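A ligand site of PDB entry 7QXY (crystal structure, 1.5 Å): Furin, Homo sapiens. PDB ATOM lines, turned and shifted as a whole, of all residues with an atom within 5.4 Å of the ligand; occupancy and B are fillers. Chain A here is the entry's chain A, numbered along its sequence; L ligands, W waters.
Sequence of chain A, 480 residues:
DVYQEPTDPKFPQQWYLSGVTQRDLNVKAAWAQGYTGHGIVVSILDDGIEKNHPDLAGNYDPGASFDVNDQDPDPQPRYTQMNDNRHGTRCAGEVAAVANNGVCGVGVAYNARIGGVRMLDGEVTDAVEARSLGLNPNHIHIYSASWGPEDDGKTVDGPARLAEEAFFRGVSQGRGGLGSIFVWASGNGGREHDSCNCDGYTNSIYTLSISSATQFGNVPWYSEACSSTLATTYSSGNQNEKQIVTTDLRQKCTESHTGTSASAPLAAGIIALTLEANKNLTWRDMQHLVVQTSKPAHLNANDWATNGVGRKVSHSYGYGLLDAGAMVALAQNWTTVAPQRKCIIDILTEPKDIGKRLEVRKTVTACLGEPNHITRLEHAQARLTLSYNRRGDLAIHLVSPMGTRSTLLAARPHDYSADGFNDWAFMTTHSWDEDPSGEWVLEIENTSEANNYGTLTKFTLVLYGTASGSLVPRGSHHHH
Residues that only touch the ligand: Leu 45 (3.3 Å), Trp 147 (3.3 Å), Val 124 (3.4 Å), Gly 148 (3.4 Å), Gly 158 (3.5 Å), Asp 157 (3.5 Å), Ala 160 (3.5 Å), Met 119 (3.5 Å), His 87 (3.6 Å), Asp 126 (3.7 Å), Leu 133 (3.7 Å), Asp 84 (3.7 Å), Trp 184 (3.7 Å), Leu 120 (3.8 Å), Ala 145 (3.8 Å) and Pro 149 (3.96 Å). 18 residues have an atom within 4 Å of the ligand: Leu 45, Asp 84, His 87, Met 119, Leu 120, Val 124, Asp 126, Glu 129, Leu 133, Ala 145, Trp 147, Gly 148, Pro 149, Asp 157, Gly 158, Ala 160, Trp 184 and Tyr 201.
The side-chain hydroxyl (OH) of Tyr 201 is in hydrogen-bond range of a nitrogen (N6) of the ligand, 3.1 Å away. OE2 of Glu 129 lies within salt-bridge range of N6 of the ligand, at 2.8 Å.
Water W6 bridges an oxygen (O4) of the ligand (2.6 Å) and the guanidinium group of Arg 86 (2.9 Å). Water W7 lies within hydrogen-bond range of an oxygen (O2) of the ligand and the backbone NH (N) of Asp 126. Water W3 bridges the backbone carbonyl oxygen of Leu 120 (2.6 Å) and a nitrogen (N3) of the ligand (2.9 Å). Water W2 lies within hydrogen-bond range of OD1 of Asp 46, OD2 of Asp 47 and N5 of the ligand. Water W1 lies within hydrogen-bond range of a nitrogen (N7) of the ligand (3.0 Å) and the side-chain carboxylate (OD1) of Asp 157 (3.1 Å).
The backbone NH of Met 119 lies within hydrogen-bond range of the backbone carbonyl oxygen of Asp 46. The side-chain carboxylate (OE1) of Glu 129 is in hydrogen-bond range of the side-chain hydroxyl (OH) of Tyr 201, at 2.5 Å. O of Trp 147 lies within hydrogen-bond range of NE1 of Trp 184, 3.0 Å away. The backbone NH (N) of Leu 120 sits at hydrogen-bond distance from the backbone carbonyl oxygen (O) of Asp 46. The side-chain sulfur (SD) of Met 119 sits close to the side-chain hydroxyl (OG) of Ser 132 (3.6 Å). The side-chain carboxylate (OD2) of Asp 47 sits at hydrogen-bond distance from the backbone NH (N) of His 87. The indole nitrogen (NE1) of Trp 147 sits at hydrogen-bond distance from the side-chain carboxylate (OD2) of Asp 46. The side-chain carboxylate (OD2) of Asp 46 is in hydrogen-bond range of a ring nitrogen (ND1) of His 87.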
ATOM      1  N   LEU A  45     -22.317 -16.281 -14.164  1.00  0.00           N
ATOM      2  CA  LEU A  45     -23.070 -15.761 -15.303  1.00  0.00           C
ATOM      3  C   LEU A  45     -22.158 -15.836 -16.499  1.00  0.00           C
ATOM      4  O   LEU A  45     -21.200 -15.068 -16.587  1.00  0.00           O
ATOM      5  CB  LEU A  45     -23.498 -14.279 -15.031  1.00  0.00           C
ATOM      6  CG  LEU A  45     -24.213 -14.001 -13.711  1.00  0.00           C
ATOM      7  CD1 LEU A  45     -24.802 -12.584 -13.715  1.00  0.00           C
ATOM      8  CD2 LEU A  45     -25.284 -14.964 -13.425  1.00  0.00           C
ATOM      9  N   ASP A  46     -22.375 -16.835 -17.389  1.00  0.00           N
ATOM     10  CA  ASP A  46     -21.431 -17.034 -18.497  1.00  0.00           C
ATOM     11  C   ASP A  46     -22.074 -17.823 -19.651  1.00  0.00           C
ATOM     12  O   ASP A  46     -23.238 -17.559 -19.944  1.00  0.00           O
ATOM     13  CB  ASP A  46     -20.135 -17.683 -17.902  1.00  0.00           C
ATOM     14  CG  ASP A  46     -18.866 -17.363 -18.653  1.00  0.00           C
ATOM     15  OD1 ASP A  46     -18.826 -17.605 -19.866  1.00  0.00           O
ATOM     16  OD2 ASP A  46     -17.904 -16.910 -18.005  1.00  0.00           O
ATOM     17  N   ASP A  47     -21.346 -18.749 -20.301  1.00  0.00           N
ATOM     18  CA  ASP A  47     -21.827 -19.525 -21.455  1.00  0.00           C
ATOM     19  C   ASP A  47     -22.359 -20.912 -21.067  1.00  0.00           C
ATOM     20  O   ASP A  47     -22.555 -21.732 -21.962  1.00  0.00           O
ATOM     21  CB  ASP A  47     -20.668 -19.682 -22.476  1.00  0.00           C
ATOM     22  CG  ASP A  47     -19.374 -20.209 -21.849  1.00  0.00           C
ATOM     23  OD1 ASP A  47     -19.441 -20.793 -20.742  1.00  0.00           O
ATOM     24  OD2 ASP A  47     -18.287 -19.970 -22.436  1.00  0.00           O
ATOM     25  N   ASN A  83     -14.835 -26.081 -28.844  1.00  0.00           N
ATOM     26  CA  ASN A  83     -14.952 -25.961 -27.384  1.00  0.00           C
ATOM     27  C   ASN A  83     -15.181 -24.504 -26.982  1.00  0.00           C
ATOM     28  O   ASN A  83     -14.583 -24.018 -26.020  1.00  0.00           O
ATOM     29  CB  ASN A  83     -13.747 -26.589 -26.664  1.00  0.00           C
ATOM     30  CG  ASN A  83     -13.741 -28.093 -26.824  1.00  0.00           C
ATOM     31  OD1 ASN A  83     -14.780 -28.743 -26.709  1.00  0.00           O
ATOM     32  ND2 ASN A  83     -12.572 -28.694 -27.089  1.00  0.00           N
ATOM     33  N   ASP A  84     -16.044 -23.801 -27.728  1.00  0.00           N
ATOM     34  CA  ASP A  84     -16.333 -22.385 -27.511  1.00  0.00           C
ATOM     35  C   ASP A  84     -17.043 -22.046 -26.199  1.00  0.00           C
ATOM     36  O   ASP A  84     -16.877 -20.923 -25.707  1.00  0.00           O
ATOM     37  CB  ASP A  84     -17.225 -21.833 -28.657  1.00  0.00           C
ATOM     38  CG  ASP A  84     -16.532 -21.695 -29.993  1.00  0.00           C
ATOM     39  N   ARG A  86     -16.808 -23.164 -23.010  1.00  0.00           N
ATOM     40  CA  ARG A  86     -16.126 -23.777 -21.871  1.00  0.00           C
ATOM     41  C   ARG A  86     -15.869 -22.846 -20.707  1.00  0.00           C
ATOM     42  O   ARG A  86     -15.486 -23.325 -19.634  1.00  0.00           O
ATOM     43  CB  ARG A  86     -14.777 -24.361 -22.337  1.00  0.00           C
ATOM     44  CG  ARG A  86     -13.736 -23.309 -22.677  1.00  0.00           C
ATOM     45  CD  ARG A  86     -12.547 -23.892 -23.381  1.00  0.00           C
ATOM     46  NE  ARG A  86     -11.538 -22.863 -23.573  1.00  0.00           N
ATOM     47  CZ  ARG A  86     -10.364 -23.059 -24.183  1.00  0.00           C
ATOM     48  NH1 ARG A  86     -10.037 -24.267 -24.644  1.00  0.00           N
ATOM     49  NH2 ARG A  86      -9.505 -22.057 -24.296  1.00  0.00           N
ATOM     50  N   HIS A  87     -15.992 -21.525 -20.912  1.00  0.00           N
ATOM     51  CA  HIS A  87     -15.590 -20.585 -19.873  1.00  0.00           C
ATOM     52  C   HIS A  87     -16.351 -20.707 -18.553  1.00  0.00           C
ATOM     53  O   HIS A  87     -15.730 -20.646 -17.491  1.00  0.00           O
ATOM     54  CB  HIS A  87     -15.639 -19.157 -20.406  1.00  0.00           C
ATOM     55  CG  HIS A  87     -14.803 -18.244 -19.572  1.00  0.00           C
ATOM     56  ND1 HIS A  87     -15.358 -17.514 -18.520  1.00  0.00           N
ATOM     57  CD2 HIS A  87     -13.467 -17.999 -19.624  1.00  0.00           C
ATOM     58  CE1 HIS A  87     -14.345 -16.854 -17.979  1.00  0.00           C
ATOM     59  NE2 HIS A  87     -13.203 -17.095 -18.622  1.00  0.00           N
ATOM     60  N   MET A 119     -26.087 -17.476 -20.351  1.00  0.00           N
ATOM     61  CA  MET A 119     -26.611 -16.195 -20.850  1.00  0.00           C
ATOM     62  C   MET A 119     -25.785 -15.598 -21.995  1.00  0.00           C
ATOM     63  O   MET A 119     -26.284 -14.700 -22.679  1.00  0.00           O
ATOM     64  CB  MET A 119     -26.669 -15.179 -19.672  1.00  0.00           C
ATOM     65  CG  MET A 119     -25.246 -14.714 -19.185  1.00  0.00           C
ATOM     66  SD  MET A 119     -25.317 -13.396 -18.012  1.00  0.00           S
ATOM     67  CE  MET A 119     -25.923 -12.075 -19.105  1.00  0.00           C
ATOM     68  N   LEU A 120     -24.534 -16.048 -22.196  1.00  0.00           N
ATOM     69  CA  LEU A 120     -23.681 -15.458 -23.243  1.00  0.00           C
ATOM     70  C   LEU A 120     -23.656 -16.227 -24.564  1.00  0.00           C
ATOM     71  O   LEU A 120     -22.982 -15.778 -25.496  1.00  0.00           O
ATOM     72  CB  LEU A 120     -22.240 -15.346 -22.733  1.00  0.00           C
ATOM     73  CG  LEU A 120     -22.036 -14.512 -21.454  1.00  0.00           C
ATOM     74  CD1 LEU A 120     -20.555 -14.443 -21.090  1.00  0.00           C
ATOM     75  CD2 LEU A 120     -22.548 -13.082 -21.625  1.00  0.00           C
ATOM     76  N   VAL A 124     -27.000 -10.965 -26.224  1.00  0.00           N
ATOM     77  CA  VAL A 124     -27.104 -10.452 -24.864  1.00  0.00           C
ATOM     78  C   VAL A 124     -27.864  -9.132 -24.920  1.00  0.00           C
ATOM     79  O   VAL A 124     -27.337  -8.138 -25.408  1.00  0.00           O
ATOM     80  CB  VAL A 124     -25.719 -10.249 -24.234  1.00  0.00           C
ATOM     81  CG1 VAL A 124     -25.863  -9.668 -22.821  1.00  0.00           C
ATOM     82  CG2 VAL A 124     -24.951 -11.560 -24.222  1.00  0.00           C
ATOM     83  N   THR A 125     -29.134  -9.173 -24.544  1.00  0.00           N
ATOM     84  CA  THR A 125     -29.994  -7.998 -24.492  1.00  0.00           C
ATOM     85  C   THR A 125     -30.152  -7.539 -23.040  1.00  0.00           C
ATOM     86  O   THR A 125     -29.794  -8.266 -22.109  1.00  0.00           O
ATOM     87  CB  THR A 125     -31.379  -8.387 -25.050  1.00  0.00           C
ATOM     88  OG1 THR A 125     -31.976  -9.333 -24.164  1.00  0.00           O
ATOM     89  CG2 THR A 125     -31.327  -8.917 -26.472  1.00  0.00           C
ATOM     90  N   ASP A 126     -30.780  -6.374 -22.833  1.00  0.00           N
ATOM     91  CA  ASP A 126     -31.058  -5.882 -21.493  1.00  0.00           C
ATOM     92  C   ASP A 126     -31.932  -6.879 -20.729  1.00  0.00           C
ATOM     93  O   ASP A 126     -31.670  -7.141 -19.568  1.00  0.00           O
ATOM     94  CB  ASP A 126     -31.764  -4.524 -21.624  1.00  0.00           C
ATOM     95  CG  ASP A 126     -32.081  -3.822 -20.336  1.00  0.00           C
ATOM     96  OD1 ASP A 126     -31.277  -3.944 -19.365  1.00  0.00           O
ATOM     97  OD2 ASP A 126     -33.107  -3.091 -20.307  1.00  0.00           O
ATOM     98  N   GLU A 129     -29.834  -9.856 -19.588  1.00  0.00           N
ATOM     99  CA  GLU A 129     -29.001  -9.471 -18.442  1.00  0.00           C
ATOM    100  C   GLU A 129     -29.837  -9.375 -17.170  1.00  0.00           C
ATOM    101  O   GLU A 129     -29.389  -9.835 -16.115  1.00  0.00           O
ATOM    102  CB  GLU A 129     -28.364  -8.098 -18.697  1.00  0.00           C
ATOM    103  CG  GLU A 129     -27.442  -8.100 -19.900  1.00  0.00           C
ATOM    104  CD  GLU A 129     -26.773  -6.765 -20.143  1.00  0.00           C
ATOM    105  OE1 GLU A 129     -26.893  -5.861 -19.289  1.00  0.00           O
ATOM    106  OE2 GLU A 129     -26.159  -6.609 -21.217  1.00  0.00           O
ATOM    107  N   SER A 132     -30.765 -12.699 -15.686  1.00  0.00           N
ATOM    108  CA  SER A 132     -29.610 -13.405 -15.132  1.00  0.00           C
ATOM    109  C   SER A 132     -29.220 -12.841 -13.771  1.00  0.00           C
ATOM    110  O   SER A 132     -29.048 -13.588 -12.813  1.00  0.00           O
ATOM    111  CB  SER A 132     -28.426 -13.283 -16.090  1.00  0.00           C
ATOM    112  OG  SER A 132     -28.811 -13.804 -17.354  1.00  0.00           O
ATOM    113  N   LEU A 133     -29.070 -11.507 -13.699  1.00  0.00           N
ATOM    114  CA  LEU A 133     -28.739 -10.820 -12.450  1.00  0.00           C
ATOM    115  C   LEU A 133     -29.817 -11.023 -11.387  1.00  0.00           C
ATOM    116  O   LEU A 133     -29.511 -11.036 -10.188  1.00  0.00           O
ATOM    117  CB  LEU A 133     -28.582  -9.308 -12.717  1.00  0.00           C
ATOM    118  CG  LEU A 133     -27.384  -8.921 -13.589  1.00  0.00           C
ATOM    119  CD1 LEU A 133     -27.525  -7.456 -14.068  1.00  0.00           C
ATOM    120  CD2 LEU A 133     -26.064  -9.106 -12.829  1.00  0.00           C
ATOM    121  N   ALA A 145     -19.473 -12.515 -12.502  1.00  0.00           N
ATOM    122  CA  ALA A 145     -19.555 -12.205 -13.944  1.00  0.00           C
ATOM    123  C   ALA A 145     -18.171 -11.755 -14.397  1.00  0.00           C
ATOM    124  O   ALA A 145     -17.603 -10.854 -13.810  1.00  0.00           O
ATOM    125  CB  ALA A 145     -20.567 -11.102 -14.195  1.00  0.00           C
ATOM    126  N   SER A 146     -17.629 -12.413 -15.415  1.00  0.00           N
ATOM    127  CA  SER A 146     -16.284 -12.139 -15.888  1.00  0.00           C
ATOM    128  C   SER A 146     -16.215 -11.262 -17.140  1.00  0.00           C
ATOM    129  O   SER A 146     -15.115 -10.970 -17.620  1.00  0.00           O
ATOM    130  CB  SER A 146     -15.633 -13.501 -16.176  1.00  0.00           C
ATOM    131  OG  SER A 146     -15.274 -14.155 -14.965  1.00  0.00           O
ATOM    132  N   TRP A 147     -17.366 -10.825 -17.666  1.00  0.00           N
ATOM    133  CA  TRP A 147     -17.429 -10.119 -18.947  1.00  0.00           C
ATOM    134  C   TRP A 147     -18.387  -8.936 -18.913  1.00  0.00           C
ATOM    135  O   TRP A 147     -19.170  -8.761 -17.978  1.00  0.00           O
ATOM    136  CB  TRP A 147     -17.911 -11.144 -20.012  1.00  0.00           C
ATOM    137  CG  TRP A 147     -17.212 -12.466 -19.979  1.00  0.00           C
ATOM    138  CD1 TRP A 147     -17.673 -13.634 -19.449  1.00  0.00           C
ATOM    139  CD2 TRP A 147     -15.892 -12.754 -20.479  1.00  0.00           C
ATOM    140  NE1 TRP A 147     -16.738 -14.631 -19.602  1.00  0.00           N
ATOM    141  CE2 TRP A 147     -15.643 -14.118 -20.253  1.00  0.00           C
ATOM    142  CE3 TRP A 147     -14.924 -12.002 -21.164  1.00  0.00           C
ATOM    143  CZ2 TRP A 147     -14.461 -14.750 -20.661  1.00  0.00           C
ATOM    144  CZ3 TRP A 147     -13.761 -12.617 -21.573  1.00  0.00           C
ATOM    145  CH2 TRP A 147     -13.545 -13.982 -21.346  1.00  0.00           C
ATOM    146  N   GLY A 148     -18.347  -8.135 -19.966  1.00  0.00           N
ATOM    147  CA  GLY A 148     -19.208  -6.968 -20.069  1.00  0.00           C
ATOM    148  C   GLY A 148     -19.113  -6.399 -21.463  1.00  0.00           C
ATOM    149  O   GLY A 148     -18.846  -7.117 -22.432  1.00  0.00           O
ATOM    150  N   PRO A 149     -19.275  -5.077 -21.589  1.00  0.00           N
ATOM    151  CA  PRO A 149     -19.168  -4.443 -22.906  1.00  0.00           C
ATOM    152  C   PRO A 149     -17.809  -4.695 -23.553  1.00  0.00           C
ATOM    153  O   PRO A 149     -16.824  -4.949 -22.865  1.00  0.00           O
ATOM    154  CB  PRO A 149     -19.339  -2.947 -22.612  1.00  0.00           C
ATOM    155  CG  PRO A 149     -19.971  -2.878 -21.288  1.00  0.00           C
ATOM    156  CD  PRO A 149     -19.588  -4.105 -20.529  1.00  0.00           C
ATOM    157  N   ASP A 157     -20.286   1.853 -22.295  1.00  0.00           N
ATOM    158  CA  ASP A 157     -21.612   1.247 -22.176  1.00  0.00           C
ATOM    159  C   ASP A 157     -21.779   0.651 -20.806  1.00  0.00           C
ATOM    160  O   ASP A 157     -20.814   0.338 -20.127  1.00  0.00           O
ATOM    161  CB  ASP A 157     -21.835   0.177 -23.268  1.00  0.00           C
ATOM    162  CG  ASP A 157     -23.287  -0.039 -23.692  1.00  0.00           C
ATOM    163  OD1 ASP A 157     -24.190   0.597 -23.097  1.00  0.00           O
ATOM    164  OD2 ASP A 157     -23.524  -0.838 -24.621  1.00  0.00           O
ATOM    165  N   GLY A 158     -23.020   0.495 -20.427  1.00  0.00           N
ATOM    166  CA  GLY A 158     -23.355  -0.028 -19.110  1.00  0.00           C
ATOM    167  C   GLY A 158     -24.723  -0.658 -19.113  1.00  0.00           C
ATOM    168  O   GLY A 158     -25.403  -0.718 -20.143  1.00  0.00           O
ATOM    169  N   PRO A 159     -25.190  -1.054 -17.924  1.00  0.00           N
ATOM    170  CA  PRO A 159     -26.512  -1.673 -17.854  1.00  0.00           C
ATOM    171  C   PRO A 159     -27.606  -0.717 -18.299  1.00  0.00           C
ATOM    172  O   PRO A 159     -27.627   0.451 -17.893  1.00  0.00           O
ATOM    173  CB  PRO A 159     -26.663  -2.039 -16.365  1.00  0.00           C
ATOM    174  CG  PRO A 159     -25.618  -1.248 -15.637  1.00  0.00           C
ATOM    175  CD  PRO A 159     -24.503  -1.032 -16.612  1.00  0.00           C
ATOM    176  N   ALA A 160     -28.479  -1.213 -19.165  1.00  0.00           N
ATOM    177  CA  ALA A 160     -29.645  -0.474 -19.608  1.00  0.00           C
ATOM    178  C   ALA A 160     -30.692  -0.591 -18.447  1.00  0.00           C
ATOM    179  O   ALA A 160     -30.363  -1.108 -17.386  1.00  0.00           O
ATOM    180  CB  ALA A 160     -30.137  -1.025 -20.951  1.00  0.00           C
ATOM    181  N   TRP A 184     -17.490  -8.753 -10.097  1.00  0.00           N
ATOM    182  CA  TRP A 184     -17.239  -8.495 -11.508  1.00  0.00           C
ATOM    183  C   TRP A 184     -15.763  -8.397 -11.811  1.00  0.00           C
ATOM    184  O   TRP A 184     -15.003  -7.900 -10.992  1.00  0.00           O
ATOM    185  CB  TRP A 184     -17.859  -7.142 -11.900  1.00  0.00           C
ATOM    186  CG  TRP A 184     -18.597  -7.167 -13.194  1.00  0.00           C
ATOM    187  CD1 TRP A 184     -18.055  -7.046 -14.448  1.00  0.00           C
ATOM    188  CD2 TRP A 184     -19.962  -7.523 -13.379  1.00  0.00           C
ATOM    189  NE1 TRP A 184     -19.029  -7.286 -15.398  1.00  0.00           N
ATOM    190  CE2 TRP A 184     -20.203  -7.606 -14.768  1.00  0.00           C
ATOM    191  CE3 TRP A 184     -21.008  -7.840 -12.488  1.00  0.00           C
ATOM    192  CZ2 TRP A 184     -21.457  -7.894 -15.292  1.00  0.00           C
ATOM    193  CZ3 TRP A 184     -22.262  -8.104 -13.017  1.00  0.00           C
ATOM    194  CH2 TRP A 184     -22.480  -8.129 -14.388  1.00  0.00           C
ATOM    195  N   TYR A 201     -20.728  -1.830 -15.780  1.00  0.00           N
ATOM    196  CA  TYR A 201     -20.968  -2.963 -14.872  1.00  0.00           C
ATOM    197  C   TYR A 201     -19.908  -2.970 -13.787  1.00  0.00           C
ATOM    198  O   TYR A 201     -20.248  -2.978 -12.609  1.00  0.00           O
ATOM    199  CB  TYR A 201     -20.969  -4.304 -15.643  1.00  0.00           C
ATOM    200  CG  TYR A 201     -22.035  -4.321 -16.699  1.00  0.00           C
ATOM    201  CD1 TYR A 201     -21.866  -3.664 -17.901  1.00  0.00           C
ATOM    202  CD2 TYR A 201     -23.262  -4.929 -16.452  1.00  0.00           C
ATOM    203  CE1 TYR A 201     -22.854  -3.655 -18.868  1.00  0.00           C
ATOM    204  CE2 TYR A 201     -24.275  -4.910 -17.408  1.00  0.00           C
ATOM    205  CZ  TYR A 201     -24.060  -4.288 -18.624  1.00  0.00           C
ATOM    206  OH  TYR A 201     -25.022  -4.236 -19.590  1.00  0.00           O
HETATM  207  N1  LIG L   1     -22.195  -8.926 -22.045  1.00  0.00           N
HETATM  208  C1  LIG L   1     -22.975  -6.272 -22.361  1.00  0.00           C
HETATM  209  C2  LIG L   1     -23.077  -6.907 -21.123  1.00  0.00           C
HETATM  210  C3  LIG L   1     -22.680  -8.233 -21.005  1.00  0.00           C
HETATM  211  C4  LIG L   1     -22.834  -8.989 -19.737  1.00  0.00           C
HETATM  212  C5  LIG L   1     -21.957 -10.023 -19.408  1.00  0.00           C
HETATM  213  C6  LIG L   1     -23.181 -10.450 -17.368  1.00  0.00           C
HETATM  214  C7  LIG L   1     -19.759 -10.250 -23.373  1.00  0.00           C
HETATM  215  C8  LIG L   1     -21.127 -11.193 -25.030  1.00  0.00           C
HETATM  216  C9  LIG L   1     -16.239 -14.160 -24.016  1.00  0.00           C
HETATM  217  C10 LIG L   1     -17.666 -15.306 -25.551  1.00  0.00           C
HETATM  218  C11 LIG L   1     -23.374  -4.838 -22.527  1.00  0.00           C
HETATM  219  C12 LIG L   1     -24.025  -9.422 -17.709  1.00  0.00           C
HETATM  220  C13 LIG L   1     -23.869  -8.680 -18.852  1.00  0.00           C
HETATM  221  C14 LIG L   1     -20.853 -10.129 -24.198  1.00  0.00           C
HETATM  222  C15 LIG L   1     -19.359 -12.335 -24.183  1.00  0.00           C
HETATM  223  C16 LIG L   1     -22.064  -8.288 -23.205  1.00  0.00           C
HETATM  224  C17 LIG L   1     -17.425 -13.573 -23.290  1.00  0.00           C
HETATM  225  C18 LIG L   1     -18.926 -14.667 -24.939  1.00  0.00           C
HETATM  226  C19 LIG L   1     -22.453  -6.986 -23.430  1.00  0.00           C
HETATM  227  C20 LIG L   1     -25.367  -5.265 -23.959  1.00  0.00           C
HETATM  228  C21 LIG L   1     -26.862  -5.048 -24.082  1.00  0.00           C
HETATM  229  C22 LIG L   1     -27.169  -3.556 -24.079  1.00  0.00           C
HETATM  230  C23 LIG L   1     -26.716  -2.995 -22.742  1.00  0.00           C
HETATM  231  C24 LIG L   1     -25.213  -3.178 -22.613  1.00  0.00           C
HETATM  232  C25 LIG L   1     -28.631  -3.285 -24.341  1.00  0.00           C
HETATM  233  C26 LIG L   1     -30.154  -1.374 -24.465  1.00  0.00           C
HETATM  234  C27 LIG L   1     -30.293   0.116 -24.654  1.00  0.00           C
HETATM  235  C28 LIG L   1     -15.512 -16.424 -24.825  1.00  0.00           C
HETATM  236  C29 LIG L   1     -14.738 -16.899 -23.607  1.00  0.00           C
HETATM  237  C30 LIG L   1     -13.730 -17.995 -23.876  1.00  0.00           C
HETATM  238  C31 LIG L   1     -22.161 -10.751 -18.257  1.00  0.00           C
HETATM  239  N2  LIG L   1     -19.010 -11.353 -23.334  1.00  0.00           N
HETATM  240  N3  LIG L   1     -20.400 -12.315 -25.020  1.00  0.00           N
HETATM  241  N4  LIG L   1     -18.595 -13.459 -24.166  1.00  0.00           N
HETATM  242  N5  LIG L   1     -16.665 -15.511 -24.475  1.00  0.00           N
HETATM  243  N6  LIG L   1     -24.863  -4.652 -22.681  1.00  0.00           N
HETATM  244  N7  LIG L   1     -28.912  -1.864 -24.454  1.00  0.00           N
HETATM  245  O1  LIG L   1     -21.601  -8.958 -24.296  1.00  0.00           O
HETATM  246  O2  LIG L   1     -31.121  -2.114 -24.312  1.00  0.00           O
HETATM  247  O3  LIG L   1     -13.998 -18.830 -24.771  1.00  0.00           O
HETATM  248  O4  LIG L   1     -12.701 -18.043 -23.184  1.00  0.00           O
HETATM  249 CL1  LIG L   1     -25.339  -9.014 -16.634  1.00  0.00          CL
HETATM  250 CL2  LIG L   1     -21.084 -12.058 -17.884  1.00  0.00          CL
HETATM  251  O   HOH W   1     -26.631   0.005 -24.926  1.00  0.00           O
HETATM  252  O   HOH W   2     -17.891 -17.105 -22.276  1.00  0.00           O
HETATM  253  O   HOH W   3     -22.057 -13.717 -26.867  1.00  0.00           O
HETATM  254  O   HOH W   4     -10.829 -16.547 -22.089  1.00  0.00           O
HETATM  255  O   HOH W   5     -19.839  -7.476 -26.616  1.00  0.00           O
HETATM  256  O   HOH W   6     -11.956 -20.342 -22.120  1.00  0.00           O
HETATM  257  O   HOH W   7     -31.637  -4.729 -25.206  1.00  0.00           O
